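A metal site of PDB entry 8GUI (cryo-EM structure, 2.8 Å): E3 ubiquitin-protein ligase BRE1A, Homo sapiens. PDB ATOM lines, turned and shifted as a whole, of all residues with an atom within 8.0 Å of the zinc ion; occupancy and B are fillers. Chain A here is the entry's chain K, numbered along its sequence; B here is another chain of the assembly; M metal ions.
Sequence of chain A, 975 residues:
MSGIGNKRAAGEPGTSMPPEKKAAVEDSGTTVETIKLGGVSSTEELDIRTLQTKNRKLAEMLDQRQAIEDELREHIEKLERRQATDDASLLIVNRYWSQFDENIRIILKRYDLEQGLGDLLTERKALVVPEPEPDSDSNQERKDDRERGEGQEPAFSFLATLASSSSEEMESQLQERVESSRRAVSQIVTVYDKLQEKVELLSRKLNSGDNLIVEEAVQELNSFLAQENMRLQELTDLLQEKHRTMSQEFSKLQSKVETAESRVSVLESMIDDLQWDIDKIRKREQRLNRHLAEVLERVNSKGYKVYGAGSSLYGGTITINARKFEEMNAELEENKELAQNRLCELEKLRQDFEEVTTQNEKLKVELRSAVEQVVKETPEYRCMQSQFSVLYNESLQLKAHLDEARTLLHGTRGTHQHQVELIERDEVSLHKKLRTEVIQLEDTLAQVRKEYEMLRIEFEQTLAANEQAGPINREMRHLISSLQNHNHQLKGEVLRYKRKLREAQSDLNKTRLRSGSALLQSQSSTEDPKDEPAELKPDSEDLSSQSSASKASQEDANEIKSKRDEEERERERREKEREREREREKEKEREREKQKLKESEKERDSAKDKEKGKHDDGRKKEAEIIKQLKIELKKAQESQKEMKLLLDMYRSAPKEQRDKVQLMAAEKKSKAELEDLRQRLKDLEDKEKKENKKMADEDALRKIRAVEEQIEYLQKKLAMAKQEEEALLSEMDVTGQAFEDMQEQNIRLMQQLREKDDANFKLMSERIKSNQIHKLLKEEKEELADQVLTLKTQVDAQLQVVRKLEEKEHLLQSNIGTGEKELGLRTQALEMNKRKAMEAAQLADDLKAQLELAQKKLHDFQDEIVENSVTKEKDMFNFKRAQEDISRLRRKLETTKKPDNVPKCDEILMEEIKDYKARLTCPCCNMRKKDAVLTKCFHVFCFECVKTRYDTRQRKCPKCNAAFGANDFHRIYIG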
ATOM      1  N   LEU A 934     -26.509 -14.648 -26.137  1.00  0.00           N
ATOM      2  CA  LEU A 934     -25.608 -15.703 -26.572  1.00  0.00           C
ATOM      3  C   LEU A 934     -26.198 -16.409 -27.790  1.00  0.00           C
ATOM      4  O   LEU A 934     -27.415 -16.630 -27.863  1.00  0.00           O
ATOM      5  CB  LEU A 934     -25.358 -16.714 -25.453  1.00  0.00           C
ATOM      6  CG  LEU A 934     -25.014 -16.164 -24.066  1.00  0.00           C
ATOM      7  CD1 LEU A 934     -24.666 -17.293 -23.121  1.00  0.00           C
ATOM      8  CD2 LEU A 934     -23.887 -15.168 -24.143  1.00  0.00           C
ATOM      9  N   LYS A 936     -25.201 -19.523 -28.842  1.00  0.00           N
ATOM     10  CA  LYS A 936     -25.223 -20.978 -28.686  1.00  0.00           C
ATOM     11  C   LYS A 936     -26.496 -21.444 -27.985  1.00  0.00           C
ATOM     12  O   LYS A 936     -27.303 -22.175 -28.562  1.00  0.00           O
ATOM     13  CB  LYS A 936     -23.979 -21.434 -27.931  1.00  0.00           C
ATOM     14  CG  LYS A 936     -22.671 -21.123 -28.636  1.00  0.00           C
ATOM     15  CD  LYS A 936     -22.595 -21.821 -29.981  1.00  0.00           C
ATOM     16  CE  LYS A 936     -22.504 -23.326 -29.813  1.00  0.00           C
ATOM     17  NZ  LYS A 936     -21.244 -23.732 -29.128  1.00  0.00           N
ATOM     18  N   CYS A 937     -26.688 -21.017 -26.747  1.00  0.00           N
ATOM     19  CA  CYS A 937     -27.863 -21.414 -25.974  1.00  0.00           C
ATOM     20  C   CYS A 937     -29.055 -20.499 -26.207  1.00  0.00           C
ATOM     21  O   CYS A 937     -30.151 -20.795 -25.714  1.00  0.00           O
ATOM     22  CB  CYS A 937     -27.529 -21.458 -24.482  1.00  0.00           C
ATOM     23  SG  CYS A 937     -27.127 -19.852 -23.758  1.00  0.00           S
ATOM     24  N   PHE A 938     -28.862 -19.399 -26.937  1.00  0.00           N
ATOM     25  CA  PHE A 938     -29.918 -18.448 -27.273  1.00  0.00           C
ATOM     26  C   PHE A 938     -30.614 -17.920 -26.024  1.00  0.00           C
ATOM     27  O   PHE A 938     -31.851 -17.867 -25.942  1.00  0.00           O
ATOM     28  CB  PHE A 938     -30.909 -19.058 -28.264  1.00  0.00           C
ATOM     29  CG  PHE A 938     -30.437 -19.018 -29.682  1.00  0.00           C
ATOM     30  CD1 PHE A 938     -30.298 -17.804 -30.342  1.00  0.00           C
ATOM     31  CD2 PHE A 938     -30.127 -20.193 -30.360  1.00  0.00           C
ATOM     32  CE1 PHE A 938     -29.855 -17.763 -31.650  1.00  0.00           C
ATOM     33  CE2 PHE A 938     -29.683 -20.152 -31.668  1.00  0.00           C
ATOM     34  CZ  PHE A 938     -29.549 -18.933 -32.315  1.00  0.00           C
ATOM     35  N   HIS A 939     -29.813 -17.534 -25.049  1.00  0.00           N
ATOM     36  CA  HIS A 939     -30.284 -16.875 -23.846  1.00  0.00           C
ATOM     37  C   HIS A 939     -29.771 -15.431 -23.812  1.00  0.00           C
ATOM     38  O   HIS A 939     -28.901 -15.045 -24.594  1.00  0.00           O
ATOM     39  CB  HIS A 939     -29.840 -17.630 -22.586  1.00  0.00           C
ATOM     40  CG  HIS A 939     -30.323 -19.048 -22.546  1.00  0.00           C
ATOM     41  ND1 HIS A 939     -29.614 -20.058 -21.932  1.00  0.00           N
ATOM     42  CD2 HIS A 939     -31.439 -19.631 -23.054  1.00  0.00           C
ATOM     43  CE1 HIS A 939     -30.264 -21.193 -22.054  1.00  0.00           C
ATOM     44  NE2 HIS A 939     -31.380 -20.961 -22.735  1.00  0.00           N
ATOM     45  N   VAL A 940     -30.332 -14.650 -22.901  1.00  0.00           N
ATOM     46  CA  VAL A 940     -30.100 -13.209 -22.855  1.00  0.00           C
ATOM     47  C   VAL A 940     -29.494 -12.861 -21.499  1.00  0.00           C
ATOM     48  O   VAL A 940     -29.989 -13.292 -20.452  1.00  0.00           O
ATOM     49  CB  VAL A 940     -31.407 -12.428 -23.090  1.00  0.00           C
ATOM     50  CG1 VAL A 940     -31.178 -10.939 -22.928  1.00  0.00           C
ATOM     51  CG2 VAL A 940     -31.967 -12.747 -24.465  1.00  0.00           C
ATOM     52  N   PHE A 941     -28.414 -12.089 -21.525  1.00  0.00           N
ATOM     53  CA  PHE A 941     -27.735 -11.608 -20.319  1.00  0.00           C
ATOM     54  C   PHE A 941     -27.353 -10.161 -20.552  1.00  0.00           C
ATOM     55  O   PHE A 941     -27.838  -9.506 -21.487  1.00  0.00           O
ATOM     56  CB  PHE A 941     -26.522 -12.487 -19.988  1.00  0.00           C
ATOM     57  CG  PHE A 941     -26.873 -13.921 -19.702  1.00  0.00           C
ATOM     58  CD1 PHE A 941     -26.888 -14.860 -20.715  1.00  0.00           C
ATOM     59  CD2 PHE A 941     -27.168 -14.323 -18.410  1.00  0.00           C
ATOM     60  CE1 PHE A 941     -27.206 -16.176 -20.449  1.00  0.00           C
ATOM     61  CE2 PHE A 941     -27.487 -15.639 -18.144  1.00  0.00           C
ATOM     62  CZ  PHE A 941     -27.505 -16.570 -19.161  1.00  0.00           C
ATOM     63  N   LYS A 956     -18.692 -20.085 -20.381  1.00  0.00           N
ATOM     64  CA  LYS A 956     -19.869 -20.938 -20.405  1.00  0.00           C
ATOM     65  C   LYS A 956     -21.066 -20.110 -19.951  1.00  0.00           C
ATOM     66  O   LYS A 956     -20.922 -19.092 -19.271  1.00  0.00           O
ATOM     67  CB  LYS A 956     -19.699 -22.176 -19.512  1.00  0.00           C
ATOM     68  CG  LYS A 956     -18.679 -23.171 -20.017  1.00  0.00           C
ATOM     69  CD  LYS A 956     -18.480 -24.315 -19.031  1.00  0.00           C
ATOM     70  CE  LYS A 956     -17.430 -25.293 -19.525  1.00  0.00           C
ATOM     71  NZ  LYS A 956     -16.078 -24.677 -19.566  1.00  0.00           N
ATOM     72  N   CYS A 957     -22.253 -20.558 -20.338  1.00  0.00           N
ATOM     73  CA  CYS A 957     -23.472 -19.865 -19.925  1.00  0.00           C
ATOM     74  C   CYS A 957     -23.643 -19.979 -18.409  1.00  0.00           C
ATOM     75  O   CYS A 957     -23.351 -21.030 -17.839  1.00  0.00           O
ATOM     76  CB  CYS A 957     -24.696 -20.415 -20.638  1.00  0.00           C
ATOM     77  SG  CYS A 957     -26.248 -19.695 -20.082  1.00  0.00           S
ATOM     78  N   PRO A 958     -24.085 -18.911 -17.742  1.00  0.00           N
ATOM     79  CA  PRO A 958     -24.249 -18.975 -16.292  1.00  0.00           C
ATOM     80  C   PRO A 958     -25.219 -20.045 -15.806  1.00  0.00           C
ATOM     81  O   PRO A 958     -25.093 -20.495 -14.665  1.00  0.00           O
ATOM     82  CB  PRO A 958     -24.738 -17.568 -15.935  1.00  0.00           C
ATOM     83  CG  PRO A 958     -24.166 -16.707 -16.994  1.00  0.00           C
ATOM     84  CD  PRO A 958     -24.185 -17.529 -18.250  1.00  0.00           C
ATOM     85  N   LYS A 959     -26.195 -20.453 -16.625  1.00  0.00           N
ATOM     86  CA  LYS A 959     -27.184 -21.427 -16.169  1.00  0.00           C
ATOM     87  C   LYS A 959     -27.139 -22.757 -16.911  1.00  0.00           C
ATOM     88  O   LYS A 959     -27.227 -23.804 -16.278  1.00  0.00           O
ATOM     89  CB  LYS A 959     -28.599 -20.815 -16.236  1.00  0.00           C
ATOM     90  CG  LYS A 959     -29.122 -20.449 -17.606  1.00  0.00           C
ATOM     91  CD  LYS A 959     -30.495 -19.817 -17.481  1.00  0.00           C
ATOM     92  CE  LYS A 959     -31.085 -19.449 -18.828  1.00  0.00           C
ATOM     93  NZ  LYS A 959     -30.292 -18.350 -19.438  1.00  0.00           N
ATOM     94  N   CYS A 960     -26.997 -22.767 -18.241  1.00  0.00           N
ATOM     95  CA  CYS A 960     -26.944 -24.040 -18.947  1.00  0.00           C
ATOM     96  C   CYS A 960     -25.525 -24.529 -19.187  1.00  0.00           C
ATOM     97  O   CYS A 960     -25.338 -25.632 -19.697  1.00  0.00           O
ATOM     98  CB  CYS A 960     -27.679 -23.977 -20.293  1.00  0.00           C
ATOM     99  SG  CYS A 960     -26.961 -22.871 -21.513  1.00  0.00           S
ATOM    100  N   ASN A 961     -24.523 -23.721 -18.829  1.00  0.00           N
ATOM    101  CA  ASN A 961     -23.105 -24.076 -18.947  1.00  0.00           C
ATOM    102  C   ASN A 961     -22.707 -24.424 -20.385  1.00  0.00           C
ATOM    103  O   ASN A 961     -21.829 -25.259 -20.612  1.00  0.00           O
ATOM    104  CB  ASN A 961     -22.742 -25.222 -17.998  1.00  0.00           C
ATOM    105  CG  ASN A 961     -22.174 -24.731 -16.682  1.00  0.00           C
ATOM    106  OD1 ASN A 961     -22.536 -23.663 -16.197  1.00  0.00           O
ATOM    107  ND2 ASN A 961     -21.264 -25.513 -16.114  1.00  0.00           N
ATOM    108  N   ALA A 962     -23.351 -23.781 -21.356  1.00  0.00           N
ATOM    109  CA  ALA A 962     -23.003 -24.009 -22.757  1.00  0.00           C
ATOM    110  C   ALA A 962     -21.802 -23.146 -23.132  1.00  0.00           C
ATOM    111  O   ALA A 962     -21.804 -21.928 -22.917  1.00  0.00           O
ATOM    112  CB  ALA A 962     -24.189 -23.680 -23.657  1.00  0.00           C
ATOM    113  N   ALA A 963     -20.776 -23.781 -23.694  1.00  0.00           N
ATOM    114  CA  ALA A 963     -19.567 -23.063 -24.079  1.00  0.00           C
ATOM    115  C   ALA A 963     -19.851 -22.177 -25.279  1.00  0.00           C
ATOM    116  O   ALA A 963     -20.452 -22.624 -26.270  1.00  0.00           O
ATOM    117  CB  ALA A 963     -18.446 -24.051 -24.389  1.00  0.00           C
ATOM    118  N   PHE A 964     -19.422 -20.924 -25.197  1.00  0.00           N
ATOM    119  CA  PHE A 964     -19.661 -19.949 -26.257  1.00  0.00           C
ATOM    120  C   PHE A 964     -18.350 -19.259 -26.625  1.00  0.00           C
ATOM    121  O   PHE A 964     -17.460 -19.079 -25.783  1.00  0.00           O
ATOM    122  CB  PHE A 964     -20.702 -18.907 -25.827  1.00  0.00           C
ATOM    123  CG  PHE A 964     -20.303 -18.089 -24.634  1.00  0.00           C
ATOM    124  CD1 PHE A 964     -20.535 -18.546 -23.353  1.00  0.00           C
ATOM    125  CD2 PHE A 964     -19.708 -16.844 -24.804  1.00  0.00           C
ATOM    126  CE1 PHE A 964     -20.169 -17.791 -22.259  1.00  0.00           C
ATOM    127  CE2 PHE A 964     -19.342 -16.089 -23.710  1.00  0.00           C
ATOM    128  CZ  PHE A 964     -19.575 -16.560 -22.431  1.00  0.00           C
ATOM    129  N   TYR B 999     -34.555 -16.400 -25.536  1.00  0.00           N
ATOM    130  CA  TYR B 999     -35.205 -16.662 -24.251  1.00  0.00           C
ATOM    131  C   TYR B 999     -35.085 -15.400 -23.406  1.00  0.00           C
ATOM    132  O   TYR B 999     -33.990 -15.059 -22.943  1.00  0.00           O
ATOM    133  CB  TYR B 999     -34.557 -17.868 -23.570  1.00  0.00           C
ATOM    134  CG  TYR B 999     -35.164 -18.314 -22.259  1.00  0.00           C
ATOM    135  CD1 TYR B 999     -36.419 -17.862 -21.857  1.00  0.00           C
ATOM    136  CD2 TYR B 999     -34.489 -19.194 -21.421  1.00  0.00           C
ATOM    137  CE1 TYR B 999     -36.974 -18.276 -20.653  1.00  0.00           C
ATOM    138  CE2 TYR B 999     -35.039 -19.613 -20.229  1.00  0.00           C
ATOM    139  CZ  TYR B 999     -36.271 -19.152 -19.847  1.00  0.00           C
ATOM    140  OH  TYR B 999     -36.821 -19.571 -18.655  1.00  0.00           O
HETATM  141 ZN    ZN M   1     -27.656 -20.672 -21.645  1.00  0.00          ZN
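A ring nitrogen (ND1) of His 939 sits close to the side-chain amino group (NZ) of Lys 959 (3.1 Å). The backbone NH (N) of Leu 934 lies within hydrogen-bond range of the backbone carbonyl oxygen (O) of His 939, at 2.9 Å. The backbone NH (N) of Ala 962 sits close to the side-chain sulfur (SG) of Cys 960. The backbone NH (N) of Lys 959 lies close to the side-chain sulfur (SG) of Cys 957 (3.5 Å). N of Cys 957 sits at hydrogen-bond distance from O of Ala 962, at 3.0 Å. The backbone carbonyl oxygen (O) of Cys 957 sits close to the side-chain amide oxygen (OD1) of Asn 961 (3.2 Å).
The zinc ion is bound by ND1 of His 939 (2.1 Å), SG of Cys 960 (2.3 Å), SG of Cys 957 (2.3 Å) and SG of Cys 937 (2.3 Å). The zinc ion has four donor atoms within binding distance.
Within 4 Å of the zinc ion: Cys 937, His 939, Cys 957 and Cys 960. Along chain A the residues within 4 Å of the zinc ion span positions 937 to 960.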
